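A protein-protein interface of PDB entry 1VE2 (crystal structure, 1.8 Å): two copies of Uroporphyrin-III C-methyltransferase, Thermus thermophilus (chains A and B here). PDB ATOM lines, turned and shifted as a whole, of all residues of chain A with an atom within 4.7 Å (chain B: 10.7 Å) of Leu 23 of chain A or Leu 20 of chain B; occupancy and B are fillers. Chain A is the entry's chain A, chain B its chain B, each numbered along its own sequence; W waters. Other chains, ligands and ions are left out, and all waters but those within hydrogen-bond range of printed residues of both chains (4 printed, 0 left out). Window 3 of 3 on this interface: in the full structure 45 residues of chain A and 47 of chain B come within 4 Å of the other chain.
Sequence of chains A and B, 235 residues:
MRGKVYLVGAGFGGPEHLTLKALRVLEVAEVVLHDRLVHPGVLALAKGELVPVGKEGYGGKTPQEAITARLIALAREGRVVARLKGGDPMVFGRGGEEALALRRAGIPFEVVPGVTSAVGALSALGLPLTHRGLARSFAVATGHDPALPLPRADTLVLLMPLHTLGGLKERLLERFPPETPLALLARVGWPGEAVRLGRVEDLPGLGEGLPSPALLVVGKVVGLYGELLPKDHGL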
ATOM      1  N   PRO A  15       6.968  -3.289 -30.414  1.00  0.00           N
ATOM      2  CA  PRO A  15       8.052  -4.078 -29.823  1.00  0.00           C
ATOM      3  C   PRO A  15       7.611  -5.211 -28.906  1.00  0.00           C
ATOM      4  O   PRO A  15       8.408  -6.097 -28.595  1.00  0.00           O
ATOM      5  CB  PRO A  15       8.893  -3.028 -29.100  1.00  0.00           C
ATOM      6  CG  PRO A  15       7.886  -2.007 -28.692  1.00  0.00           C
ATOM      7  CD  PRO A  15       6.991  -1.900 -29.914  1.00  0.00           C
ATOM      8  N   GLU A  16       6.349  -5.206 -28.484  1.00  0.00           N
ATOM      9  CA  GLU A  16       5.863  -6.266 -27.598  1.00  0.00           C
ATOM     10  C   GLU A  16       5.849  -7.616 -28.315  1.00  0.00           C
ATOM     11  O   GLU A  16       5.831  -8.669 -27.665  1.00  0.00           O
ATOM     12  CB  GLU A  16       4.458  -5.944 -27.088  1.00  0.00           C
ATOM     13  CG  GLU A  16       3.387  -6.074 -28.149  1.00  0.00           C
ATOM     14  CD  GLU A  16       2.139  -5.316 -27.802  1.00  0.00           C
ATOM     15  OE1 GLU A  16       1.626  -5.494 -26.675  1.00  0.00           O
ATOM     16  OE2 GLU A  16       1.667  -4.541 -28.661  1.00  0.00           O
ATOM     17  N   LEU A  18       8.283  -8.500 -30.428  1.00  0.00           N
ATOM     18  CA  LEU A  18       9.669  -8.875 -30.695  1.00  0.00           C
ATOM     19  C   LEU A  18       9.940 -10.115 -29.851  1.00  0.00           C
ATOM     20  O   LEU A  18       9.343 -10.267 -28.796  1.00  0.00           O
ATOM     21  CB  LEU A  18      10.637  -7.785 -30.227  1.00  0.00           C
ATOM     22  CG  LEU A  18      10.902  -6.576 -31.113  1.00  0.00           C
ATOM     23  CD1 LEU A  18      11.784  -5.566 -30.375  1.00  0.00           C
ATOM     24  CD2 LEU A  18      11.577  -7.055 -32.395  1.00  0.00           C
ATOM     25  N   THR A  19      10.827 -10.994 -30.300  1.00  0.00           N
ATOM     26  CA  THR A  19      11.159 -12.172 -29.500  1.00  0.00           C
ATOM     27  C   THR A  19      12.259 -11.751 -28.537  1.00  0.00           C
ATOM     28  O   THR A  19      12.868 -10.700 -28.712  1.00  0.00           O
ATOM     29  CB  THR A  19      11.696 -13.329 -30.351  1.00  0.00           C
ATOM     30  OG1 THR A  19      12.934 -12.940 -30.971  1.00  0.00           O
ATOM     31  CG2 THR A  19      10.675 -13.714 -31.413  1.00  0.00           C
ATOM     32  N   LEU A  20      12.527 -12.575 -27.533  1.00  0.00           N
ATOM     33  CA  LEU A  20      13.552 -12.236 -26.550  1.00  0.00           C
ATOM     34  C   LEU A  20      14.944 -12.147 -27.174  1.00  0.00           C
ATOM     35  O   LEU A  20      15.747 -11.298 -26.777  1.00  0.00           O
ATOM     36  CB  LEU A  20      13.543 -13.262 -25.406  1.00  0.00           C
ATOM     37  CG  LEU A  20      12.202 -13.458 -24.681  1.00  0.00           C
ATOM     38  CD1 LEU A  20      12.432 -14.260 -23.401  1.00  0.00           C
ATOM     39  CD2 LEU A  20      11.576 -12.108 -24.338  1.00  0.00           C
ATOM     40  N   LYS A  21      15.230 -13.018 -28.139  1.00  0.00           N
ATOM     41  CA  LYS A  21      16.529 -13.009 -28.811  1.00  0.00           C
ATOM     42  C   LYS A  21      16.662 -11.727 -29.620  1.00  0.00           C
ATOM     43  O   LYS A  21      17.711 -11.076 -29.619  1.00  0.00           O
ATOM     44  CB  LYS A  21      16.672 -14.218 -29.747  1.00  0.00           C
ATOM     45  CG  LYS A  21      18.064 -14.339 -30.359  1.00  0.00           C
ATOM     46  CD  LYS A  21      18.259 -15.666 -31.056  1.00  0.00           C
ATOM     47  CE  LYS A  21      19.652 -15.764 -31.657  1.00  0.00           C
ATOM     48  NZ  LYS A  21      19.890 -17.082 -32.330  1.00  0.00           N
ATOM     49  N   ALA A  22      15.594 -11.369 -30.326  1.00  0.00           N
ATOM     50  CA  ALA A  22      15.624 -10.155 -31.132  1.00  0.00           C
ATOM     51  C   ALA A  22      15.964  -8.958 -30.234  1.00  0.00           C
ATOM     52  O   ALA A  22      16.757  -8.092 -30.609  1.00  0.00           O
ATOM     53  CB  ALA A  22      14.277  -9.956 -31.821  1.00  0.00           C
ATOM     54  N   LEU A  23      15.369  -8.920 -29.047  1.00  0.00           N
ATOM     55  CA  LEU A  23      15.631  -7.838 -28.102  1.00  0.00           C
ATOM     56  C   LEU A  23      17.112  -7.795 -27.744  1.00  0.00           C
ATOM     57  O   LEU A  23      17.727  -6.736 -27.759  1.00  0.00           O
ATOM     58  CB  LEU A  23      14.817  -8.036 -26.820  1.00  0.00           C
ATOM     59  CG  LEU A  23      13.300  -7.895 -26.895  1.00  0.00           C
ATOM     60  CD1 LEU A  23      12.688  -8.320 -25.562  1.00  0.00           C
ATOM     61  CD2 LEU A  23      12.941  -6.451 -27.208  1.00  0.00           C
ATOM     62  N   ARG A  24      17.686  -8.949 -27.422  1.00  0.00           N
ATOM     63  CA  ARG A  24      19.094  -8.982 -27.052  1.00  0.00           C
ATOM     64  C   ARG A  24      19.969  -8.482 -28.184  1.00  0.00           C
ATOM     65  O   ARG A  24      20.871  -7.674 -27.965  1.00  0.00           O
ATOM     66  CB  ARG A  24      19.542 -10.396 -26.660  1.00  0.00           C
ATOM     67  CG  ARG A  24      21.036 -10.464 -26.306  1.00  0.00           C
ATOM     68  CD  ARG A  24      21.489 -11.865 -25.898  1.00  0.00           C
ATOM     69  NE  ARG A  24      21.485 -12.819 -27.010  1.00  0.00           N
ATOM     70  CZ  ARG A  24      22.332 -12.782 -28.038  1.00  0.00           C
ATOM     71  NH1 ARG A  24      23.260 -11.836 -28.108  1.00  0.00           N
ATOM     72  NH2 ARG A  24      22.257 -13.697 -28.995  1.00  0.00           N
ATOM     73  N   VAL A  25      19.707  -8.962 -29.397  1.00  0.00           N
ATOM     74  CA  VAL A  25      20.491  -8.544 -30.547  1.00  0.00           C
ATOM     75  C   VAL A  25      20.437  -7.036 -30.763  1.00  0.00           C
ATOM     76  O   VAL A  25      21.459  -6.423 -31.050  1.00  0.00           O
ATOM     77  CB  VAL A  25      20.027  -9.252 -31.840  1.00  0.00           C
ATOM     78  CG1 VAL A  25      20.737  -8.641 -33.058  1.00  0.00           C
ATOM     79  CG2 VAL A  25      20.319 -10.741 -31.737  1.00  0.00           C
ATOM     80  N   LEU A  26      19.254  -6.439 -30.628  1.00  0.00           N
ATOM     81  CA  LEU A  26      19.119  -4.998 -30.825  1.00  0.00           C
ATOM     82  C   LEU A  26      19.852  -4.197 -29.756  1.00  0.00           C
ATOM     83  O   LEU A  26      20.120  -3.009 -29.936  1.00  0.00           O
ATOM     84  CB  LEU A  26      17.644  -4.590 -30.860  1.00  0.00           C
ATOM     85  CG  LEU A  26      16.875  -5.120 -32.078  1.00  0.00           C
ATOM     86  CD1 LEU A  26      15.446  -4.593 -32.074  1.00  0.00           C
ATOM     87  CD2 LEU A  26      17.599  -4.688 -33.347  1.00  0.00           C
ATOM     88  N   GLU A  27      20.183  -4.846 -28.647  1.00  0.00           N
ATOM     89  CA  GLU A  27      20.903  -4.171 -27.575  1.00  0.00           C
ATOM     90  C   GLU A  27      22.405  -4.198 -27.828  1.00  0.00           C
ATOM     91  O   GLU A  27      23.097  -3.204 -27.609  1.00  0.00           O
ATOM     92  CB  GLU A  27      20.623  -4.843 -26.234  1.00  0.00           C
ATOM     93  CG  GLU A  27      19.162  -4.944 -25.894  1.00  0.00           C
ATOM     94  CD  GLU A  27      18.932  -5.509 -24.516  1.00  0.00           C
ATOM     95  OE1 GLU A  27      19.451  -6.606 -24.216  1.00  0.00           O
ATOM     96  OE2 GLU A  27      18.230  -4.849 -23.726  1.00  0.00           O
ATOM     97  N   LEU A  45      14.504   0.545 -29.305  1.00  0.00           N
ATOM     98  CA  LEU A  45      15.207  -0.438 -28.484  1.00  0.00           C
ATOM     99  C   LEU A  45      16.622  -0.754 -28.977  1.00  0.00           C
ATOM    100  O   LEU A  45      17.400  -1.412 -28.283  1.00  0.00           O
ATOM    101  CB  LEU A  45      14.385  -1.720 -28.394  1.00  0.00           C
ATOM    102  CG  LEU A  45      13.191  -1.594 -27.445  1.00  0.00           C
ATOM    103  CD1 LEU A  45      12.167  -2.695 -27.712  1.00  0.00           C
ATOM    104  CD2 LEU A  45      13.709  -1.660 -26.005  1.00  0.00           C
ATOM    105  N   TYR B   6      -5.979 -15.528 -22.062  1.00  0.00           N
ATOM    106  CA  TYR B   6      -4.989 -15.199 -23.078  1.00  0.00           C
ATOM    107  C   TYR B   6      -4.674 -16.470 -23.852  1.00  0.00           C
ATOM    108  O   TYR B   6      -4.326 -17.486 -23.256  1.00  0.00           O
ATOM    109  CB  TYR B   6      -3.699 -14.682 -22.442  1.00  0.00           C
ATOM    110  CG  TYR B   6      -3.787 -13.268 -21.918  1.00  0.00           C
ATOM    111  CD1 TYR B   6      -3.699 -12.173 -22.785  1.00  0.00           C
ATOM    112  CD2 TYR B   6      -3.988 -13.019 -20.560  1.00  0.00           C
ATOM    113  CE1 TYR B   6      -3.808 -10.866 -22.311  1.00  0.00           C
ATOM    114  CE2 TYR B   6      -4.101 -11.715 -20.077  1.00  0.00           C
ATOM    115  CZ  TYR B   6      -4.010 -10.645 -20.958  1.00  0.00           C
ATOM    116  OH  TYR B   6      -4.117  -9.355 -20.486  1.00  0.00           O
ATOM    117  N   VAL B   8      -2.089 -17.849 -25.776  1.00  0.00           N
ATOM    118  CA  VAL B   8      -0.678 -17.531 -26.004  1.00  0.00           C
ATOM    119  C   VAL B   8       0.166 -18.544 -26.775  1.00  0.00           C
ATOM    120  O   VAL B   8       0.121 -19.739 -26.507  1.00  0.00           O
ATOM    121  CB  VAL B   8       0.038 -17.279 -24.653  1.00  0.00           C
ATOM    122  CG1 VAL B   8       1.447 -16.760 -24.894  1.00  0.00           C
ATOM    123  CG2 VAL B   8      -0.764 -16.308 -23.809  1.00  0.00           C
ATOM    124  N   GLY B   9       0.948 -18.042 -27.728  1.00  0.00           N
ATOM    125  CA  GLY B   9       1.828 -18.900 -28.498  1.00  0.00           C
ATOM    126  C   GLY B   9       3.158 -18.970 -27.777  1.00  0.00           C
ATOM    127  O   GLY B   9       3.679 -17.953 -27.323  1.00  0.00           O
ATOM    128  N   ALA B  10       3.709 -20.174 -27.658  1.00  0.00           N
ATOM    129  CA  ALA B  10       4.980 -20.366 -26.984  1.00  0.00           C
ATOM    130  C   ALA B  10       6.149 -20.341 -27.965  1.00  0.00           C
ATOM    131  O   ALA B  10       7.309 -20.425 -27.556  1.00  0.00           O
ATOM    132  CB  ALA B  10       4.968 -21.701 -26.238  1.00  0.00           C
ATOM    133  N   GLY B  11       5.858 -20.213 -29.257  1.00  0.00           N
ATOM    134  CA  GLY B  11       6.948 -20.244 -30.219  1.00  0.00           C
ATOM    135  C   GLY B  11       7.256 -21.719 -30.459  1.00  0.00           C
ATOM    136  O   GLY B  11       6.741 -22.581 -29.745  1.00  0.00           O
ATOM    137  N   GLY B  14      12.763 -22.968 -27.739  1.00  0.00           N
ATOM    138  CA  GLY B  14      13.155 -22.398 -26.465  1.00  0.00           C
ATOM    139  C   GLY B  14      12.599 -21.025 -26.147  1.00  0.00           C
ATOM    140  O   GLY B  14      11.995 -20.371 -26.993  1.00  0.00           O
ATOM    141  N   PRO B  15      12.803 -20.556 -24.911  1.00  0.00           N
ATOM    142  CA  PRO B  15      12.315 -19.242 -24.489  1.00  0.00           C
ATOM    143  C   PRO B  15      12.888 -18.077 -25.295  1.00  0.00           C
ATOM    144  O   PRO B  15      12.285 -17.003 -25.349  1.00  0.00           O
ATOM    145  CB  PRO B  15      12.688 -19.196 -23.004  1.00  0.00           C
ATOM    146  CG  PRO B  15      13.884 -20.090 -22.914  1.00  0.00           C
ATOM    147  CD  PRO B  15      13.497 -21.243 -23.809  1.00  0.00           C
ATOM    148  N   GLU B  16      14.035 -18.287 -25.938  1.00  0.00           N
ATOM    149  CA  GLU B  16      14.651 -17.230 -26.734  1.00  0.00           C
ATOM    150  C   GLU B  16      13.747 -16.758 -27.879  1.00  0.00           C
ATOM    151  O   GLU B  16      13.894 -15.637 -28.370  1.00  0.00           O
ATOM    152  CB  GLU B  16      16.002 -17.690 -27.308  1.00  0.00           C
ATOM    153  CG  GLU B  16      15.912 -18.849 -28.280  1.00  0.00           C
ATOM    154  CD  GLU B  16      16.151 -20.197 -27.622  1.00  0.00           C
ATOM    155  OE1 GLU B  16      15.803 -20.350 -26.427  1.00  0.00           O
ATOM    156  OE2 GLU B  16      16.677 -21.109 -28.307  1.00  0.00           O
ATOM    157  N   HIS B  17      12.813 -17.605 -28.303  1.00  0.00           N
ATOM    158  CA  HIS B  17      11.907 -17.244 -29.390  1.00  0.00           C
ATOM    159  C   HIS B  17      10.519 -16.825 -28.925  1.00  0.00           C
ATOM    160  O   HIS B  17       9.618 -16.611 -29.739  1.00  0.00           O
ATOM    161  CB  HIS B  17      11.810 -18.399 -30.388  1.00  0.00           C
ATOM    162  CG  HIS B  17      13.121 -18.740 -31.021  1.00  0.00           C
ATOM    163  ND1 HIS B  17      13.830 -17.840 -31.787  1.00  0.00           N
ATOM    164  CD2 HIS B  17      13.865 -19.868 -30.979  1.00  0.00           C
ATOM    165  CE1 HIS B  17      14.956 -18.401 -32.190  1.00  0.00           C
ATOM    166  NE2 HIS B  17      15.000 -19.632 -31.715  1.00  0.00           N
ATOM    167  N   LEU B  18      10.353 -16.711 -27.610  1.00  0.00           N
ATOM    168  CA  LEU B  18       9.090 -16.272 -27.022  1.00  0.00           C
ATOM    169  C   LEU B  18       9.007 -14.767 -27.279  1.00  0.00           C
ATOM    170  O   LEU B  18      10.031 -14.101 -27.268  1.00  0.00           O
ATOM    171  CB  LEU B  18       9.124 -16.466 -25.505  1.00  0.00           C
ATOM    172  CG  LEU B  18       8.233 -17.446 -24.752  1.00  0.00           C
ATOM    173  CD1 LEU B  18       8.313 -17.070 -23.265  1.00  0.00           C
ATOM    174  CD2 LEU B  18       6.801 -17.392 -25.239  1.00  0.00           C
ATOM    175  N   THR B  19       7.813 -14.226 -27.501  1.00  0.00           N
ATOM    176  CA  THR B  19       7.701 -12.777 -27.694  1.00  0.00           C
ATOM    177  C   THR B  19       7.653 -12.091 -26.328  1.00  0.00           C
ATOM    178  O   THR B  19       7.353 -12.722 -25.316  1.00  0.00           O
ATOM    179  CB  THR B  19       6.428 -12.365 -28.479  1.00  0.00           C
ATOM    180  OG1 THR B  19       5.248 -12.741 -27.755  1.00  0.00           O
ATOM    181  CG2 THR B  19       6.421 -13.014 -29.853  1.00  0.00           C
ATOM    182  N   LEU B  20       7.966 -10.801 -26.304  1.00  0.00           N
ATOM    183  CA  LEU B  20       7.941 -10.036 -25.064  1.00  0.00           C
ATOM    184  C   LEU B  20       6.564 -10.113 -24.419  1.00  0.00           C
ATOM    185  O   LEU B  20       6.441 -10.286 -23.201  1.00  0.00           O
ATOM    186  CB  LEU B  20       8.269  -8.571 -25.339  1.00  0.00           C
ATOM    187  CG  LEU B  20       9.509  -7.983 -24.675  1.00  0.00           C
ATOM    188  CD1 LEU B  20       9.537  -6.486 -24.943  1.00  0.00           C
ATOM    189  CD2 LEU B  20       9.489  -8.263 -23.177  1.00  0.00           C
ATOM    190  N   LYS B  21       5.526  -9.978 -25.243  1.00  0.00           N
ATOM    191  CA  LYS B  21       4.156 -10.017 -24.751  1.00  0.00           C
ATOM    192  C   LYS B  21       3.815 -11.372 -24.133  1.00  0.00           C
ATOM    193  O   LYS B  21       3.113 -11.438 -23.124  1.00  0.00           O
ATOM    194  CB  LYS B  21       3.172  -9.690 -25.879  1.00  0.00           C
ATOM    195  CG  LYS B  21       1.731  -9.479 -25.395  1.00  0.00           C
ATOM    196  CD  LYS B  21       0.824  -8.938 -26.493  1.00  0.00           C
ATOM    197  CE  LYS B  21      -0.559  -8.592 -25.951  1.00  0.00           C
ATOM    198  NZ  LYS B  21      -1.434  -7.976 -26.997  1.00  0.00           N
ATOM    199  N   ALA B  22       4.301 -12.455 -24.737  1.00  0.00           N
ATOM    200  CA  ALA B  22       4.026 -13.785 -24.192  1.00  0.00           C
ATOM    201  C   ALA B  22       4.752 -13.915 -22.849  1.00  0.00           C
ATOM    202  O   ALA B  22       4.246 -14.528 -21.901  1.00  0.00           O
ATOM    203  CB  ALA B  22       4.493 -14.873 -25.169  1.00  0.00           C
ATOM    204  N   LEU B  23       5.938 -13.325 -22.769  1.00  0.00           N
ATOM    205  CA  LEU B  23       6.718 -13.358 -21.540  1.00  0.00           C
ATOM    206  C   LEU B  23       5.896 -12.679 -20.444  1.00  0.00           C
ATOM    207  O   LEU B  23       5.777 -13.198 -19.336  1.00  0.00           O
ATOM    208  CB  LEU B  23       8.033 -12.602 -21.727  1.00  0.00           C
ATOM    209  CG  LEU B  23       9.260 -12.959 -20.871  1.00  0.00           C
ATOM    210  CD1 LEU B  23       9.992 -11.689 -20.485  1.00  0.00           C
ATOM    211  CD2 LEU B  23       8.862 -13.730 -19.646  1.00  0.00           C
ATOM    212  N   ARG B  24       5.313 -11.523 -20.758  1.00  0.00           N
ATOM    213  CA  ARG B  24       4.517 -10.805 -19.766  1.00  0.00           C
ATOM    214  C   ARG B  24       3.299 -11.591 -19.312  1.00  0.00           C
ATOM    215  O   ARG B  24       2.960 -11.583 -18.131  1.00  0.00           O
ATOM    216  CB  ARG B  24       4.059  -9.443 -20.300  1.00  0.00           C
ATOM    217  CG  ARG B  24       5.197  -8.488 -20.617  1.00  0.00           C
ATOM    218  CD  ARG B  24       4.689  -7.047 -20.738  1.00  0.00           C
ATOM    219  NE  ARG B  24       3.443  -6.968 -21.496  1.00  0.00           N
ATOM    220  CZ  ARG B  24       3.308  -6.380 -22.682  1.00  0.00           C
ATOM    221  NH1 ARG B  24       4.346  -5.804 -23.275  1.00  0.00           N
ATOM    222  NH2 ARG B  24       2.123  -6.365 -23.273  1.00  0.00           N
ATOM    223  N   VAL B  25       2.628 -12.258 -20.246  1.00  0.00           N
ATOM    224  CA  VAL B  25       1.451 -13.043 -19.894  1.00  0.00           C
ATOM    225  C   VAL B  25       1.858 -14.193 -18.974  1.00  0.00           C
ATOM    226  O   VAL B  25       1.146 -14.520 -18.023  1.00  0.00           O
ATOM    227  CB  VAL B  25       0.742 -13.605 -21.148  1.00  0.00           C
ATOM    228  CG1 VAL B  25      -0.286 -14.653 -20.747  1.00  0.00           C
ATOM    229  CG2 VAL B  25       0.042 -12.474 -21.898  1.00  0.00           C
ATOM    230  N   LEU B  26       3.009 -14.798 -19.240  1.00  0.00           N
ATOM    231  CA  LEU B  26       3.463 -15.903 -18.401  1.00  0.00           C
ATOM    232  C   LEU B  26       3.826 -15.427 -17.003  1.00  0.00           C
ATOM    233  O   LEU B  26       3.750 -16.192 -16.040  1.00  0.00           O
ATOM    234  CB  LEU B  26       4.663 -16.607 -19.034  1.00  0.00           C
ATOM    235  CG  LEU B  26       4.339 -17.374 -20.321  1.00  0.00           C
ATOM    236  CD1 LEU B  26       5.588 -18.068 -20.819  1.00  0.00           C
ATOM    237  CD2 LEU B  26       3.231 -18.385 -20.065  1.00  0.00           C
ATOM    238  N   GLU B  27       4.217 -14.163 -16.878  1.00  0.00           N
ATOM    239  CA  GLU B  27       4.573 -13.649 -15.564  1.00  0.00           C
ATOM    240  C   GLU B  27       3.346 -13.167 -14.786  1.00  0.00           C
ATOM    241  O   GLU B  27       3.369 -13.118 -13.557  1.00  0.00           O
ATOM    242  CB  GLU B  27       5.604 -12.524 -15.698  1.00  0.00           C
ATOM    243  CG  GLU B  27       6.835 -12.944 -16.510  1.00  0.00           C
ATOM    244  CD  GLU B  27       8.050 -12.058 -16.275  1.00  0.00           C
ATOM    245  OE1 GLU B  27       7.901 -10.816 -16.265  1.00  0.00           O
ATOM    246  OE2 GLU B  27       9.163 -12.614 -16.114  1.00  0.00           O
ATOM    247  N   VAL B  28       2.271 -12.844 -15.501  1.00  0.00           N
ATOM    248  CA  VAL B  28       1.049 -12.343 -14.879  1.00  0.00           C
ATOM    249  C   VAL B  28      -0.080 -13.368 -14.693  1.00  0.00           C
ATOM    250  O   VAL B  28      -0.830 -13.287 -13.721  1.00  0.00           O
ATOM    251  CB  VAL B  28       0.485 -11.137 -15.684  1.00  0.00           C
ATOM    252  CG1 VAL B  28      -0.772 -10.598 -15.019  1.00  0.00           C
ATOM    253  CG2 VAL B  28       1.544 -10.037 -15.789  1.00  0.00           C
ATOM    254  N   LEU B  45       9.174 -20.161 -17.149  1.00  0.00           N
ATOM    255  CA  LEU B  45       8.915 -18.733 -17.010  1.00  0.00           C
ATOM    256  C   LEU B  45       7.521 -18.429 -16.461  1.00  0.00           C
ATOM    257  O   LEU B  45       7.224 -17.291 -16.090  1.00  0.00           O
ATOM    258  CB  LEU B  45       9.114 -18.036 -18.359  1.00  0.00           C
ATOM    259  CG  LEU B  45      10.561 -18.022 -18.862  1.00  0.00           C
ATOM    260  CD1 LEU B  45      10.620 -17.487 -20.286  1.00  0.00           C
ATOM    261  CD2 LEU B  45      11.415 -17.173 -17.931  1.00  0.00           C
ATOM    262  N   VAL B 112      -2.194 -13.792 -28.253  1.00  0.00           N
ATOM    263  CA  VAL B 112      -0.797 -13.391 -28.265  1.00  0.00           C
ATOM    264  C   VAL B 112      -0.037 -14.292 -29.241  1.00  0.00           C
ATOM    265  O   VAL B 112       0.217 -15.460 -28.945  1.00  0.00           O
ATOM    266  CB  VAL B 112      -0.215 -13.531 -26.837  1.00  0.00           C
ATOM    267  CG1 VAL B 112       1.249 -13.151 -26.809  1.00  0.00           C
ATOM    268  CG2 VAL B 112      -1.029 -12.653 -25.870  1.00  0.00           C
ATOM    269  N   PRO B 113       0.323 -13.756 -30.421  1.00  0.00           N
ATOM    270  CA  PRO B 113       1.049 -14.490 -31.468  1.00  0.00           C
ATOM    271  C   PRO B 113       2.408 -15.040 -31.032  1.00  0.00           C
ATOM    272  O   PRO B 113       3.080 -14.480 -30.158  1.00  0.00           O
ATOM    273  CB  PRO B 113       1.208 -13.450 -32.587  1.00  0.00           C
ATOM    274  CG  PRO B 113       0.112 -12.469 -32.331  1.00  0.00           C
ATOM    275  CD  PRO B 113       0.078 -12.362 -30.834  1.00  0.00           C
ATOM    276  N   GLY B 114       2.811 -16.133 -31.668  1.00  0.00           N
ATOM    277  CA  GLY B 114       4.094 -16.739 -31.378  1.00  0.00           C
ATOM    278  C   GLY B 114       4.725 -17.137 -32.697  1.00  0.00           C
ATOM    279  O   GLY B 114       4.031 -17.233 -33.708  1.00  0.00           O
ATOM    280  N   VAL B 115       6.031 -17.347 -32.697  1.00  0.00           N
ATOM    281  CA  VAL B 115       6.751 -17.761 -33.893  1.00  0.00           C
ATOM    282  C   VAL B 115       6.341 -19.200 -34.229  1.00  0.00           C
ATOM    283  O   VAL B 115       6.547 -20.113 -33.432  1.00  0.00           O
ATOM    284  CB  VAL B 115       8.268 -17.699 -33.645  1.00  0.00           C
ATOM    285  CG1 VAL B 115       9.032 -18.267 -34.836  1.00  0.00           C
ATOM    286  CG2 VAL B 115       8.682 -16.254 -33.374  1.00  0.00           C
HETATM  287  O   HOH W   1       3.499  -3.206 -24.977  1.00  0.00           O
HETATM  288  O   HOH W   2      -0.620  -5.428 -28.449  1.00  0.00           O
HETATM  289  O   HOH W   3      13.743 -15.032 -32.447  1.00  0.00           O
HETATM  290  O   HOH W   4      -0.656  -4.945 -24.717  1.00  0.00           O
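Water W2 lies within hydrogen-bond range of the side-chain carboxylate (OE2) of Glu 16 of chain A (2.5 Å) and the side-chain amino group (NZ) of Lys 21 of chain B (3.0 Å).
Water W1 lies within hydrogen-bond range of NH1 of Arg 24 of chain B (3.2 Å) and OE1 of Glu 16 of chain A (3.4 Å).
O of Pro 15 of chain A touches CD1 of Leu 20 of chain B, at 3.8 Å.
Leu 18 of chain A touches Thr 19 of chain B.
Thr 19 of chain A touches Glu 16 of chain B (CB to O, 3.8 Å).
His 17 of chain B touches Thr 19 of chain A.
Leu 18 of chain B touches Thr 19 of chain A (O to CA, 3.2 Å).
Thr 19 of chain A touches Thr 19 of chain B.
CG2 of Thr 19 of chain A touches CG2 of Val 115 of chain B (3.8 Å).
Pro 15 of chain B touches Leu 20 of chain A.
Of chain B, only Leu 20 comes within 4 Å of Leu 23 of chain A.
Leu 20 of chain B touches four residues of chain A.
Of the printed residues of chain B, Leu 18 of chain A touches Thr 19 and Leu 20.
Of chain B, only Glu 16, His 17, Leu 18, Thr 19 and Val 115 come within 4 Å of Thr 19 of chain A.
Leu 20 of chain A touches just these residues of chain B: Pro 15, Glu 16 and Leu 18.
No residue of chain B comes within 4 Å of Ala 22 of chain A.
No residue of chain B comes within 4 Å of Leu 26 of chain A.
Of the printed residues of chain B, Glu 16 of chain A touches Thr 19 (3.8 Å), Leu 20 (3.3 Å), Lys 21 (2.8 Å) and Arg 24 (3.5 Å).
Of the printed residues of chain A, Lys 21 of chain B touches Glu 16 (2.8 Å).
Val 112 of chain B touches none of the printed residues of chain A.
Pro 113 of chain B touches none of the printed residues of chain A.
The nearest residue of chain A that does not touch Leu 20 of chain B is Leu 20 of chain A (4.2 Å).
The nearest printed residue of chain A that does not touch Arg 24 of chain B is Pro 15 of chain A (6.5 Å).
Of the 25 printed residues of chain B, 9 touch a printed residue of chain A.
Printed residues of chain B that touch a printed residue of chain A: Pro 15, Glu 16, His 17, Leu 18, Thr 19, Leu 20, Lys 21, Arg 24 and Val 115.
Hydrophobic or aromatic side chains of chain B within 4 Å of the printed part of chain A: Leu 20 and Val 115.
Of the 13 printed residues of chain A, 7 touch a printed residue of chain B.
Among the printed residues, 17 pairs touch across the chains.
Among the printed residues, Asp or Glu carboxylates within 4 Å of a Lys or Arg side-chain nitrogen of the other chain: Glu 16 of chain A with Lys 21 of chain B and Glu 16 of chain A with Arg 24 of chain B.
Glu 16 of chain A touches Arg 24 of chain B, but with the chains exchanged Arg 24 of chain A does not touch Glu 16 of chain B (7.3 Å).
Leu 18 of chain A touches Thr 19 of chain B, and with the chains exchanged Thr 19 of chain A touches Leu 18 of chain B.
Of the 17 pairs that touch across the chains among the printed residues, 13 have their exchanged pair printed and touching as well.
The backbone NH of Leu 20 of chain B lies within hydrogen-bond range of the backbone carbonyl oxygen of Glu 16 of chain A (3.3 Å).
The backbone carbonyl oxygen (O) of Leu 18 of chain B sits at hydrogen-bond distance from the backbone NH (N) of Leu 20 of chain A (2.9 Å).
The side-chain carboxylate (OE1) of Glu 16 of chain A lies within salt-bridge range of the side-chain amino group (NZ) of Lys 21 of chain B.
OE1 of Glu 16 of chain A is in salt-bridge range of NH2 of Arg 24 of chain B (3.5 Å).
The backbone NH (N) of Leu 20 of chain A sits at hydrogen-bond distance from the backbone carbonyl oxygen (O) of Glu 16 of chain B (3.5 Å).
The backbone carbonyl oxygen (O) of Glu 16 of chain B lies within hydrogen-bond range of the backbone NH (N) of Lys 21 of chain A (2.9 Å).
The backbone NH (N) of Leu 20 of chain B lies within hydrogen-bond range of the backbone carbonyl oxygen (O) of Leu 18 of chain A (2.9 Å).
N of Ala 22 of chain A lies within hydrogen-bond range of OG1 of Thr 19 of chain A, 3.2 Å away.
N of Ala 22 of chain B lies within hydrogen-bond range of OG1 of Thr 19 of chain B (3.2 Å).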
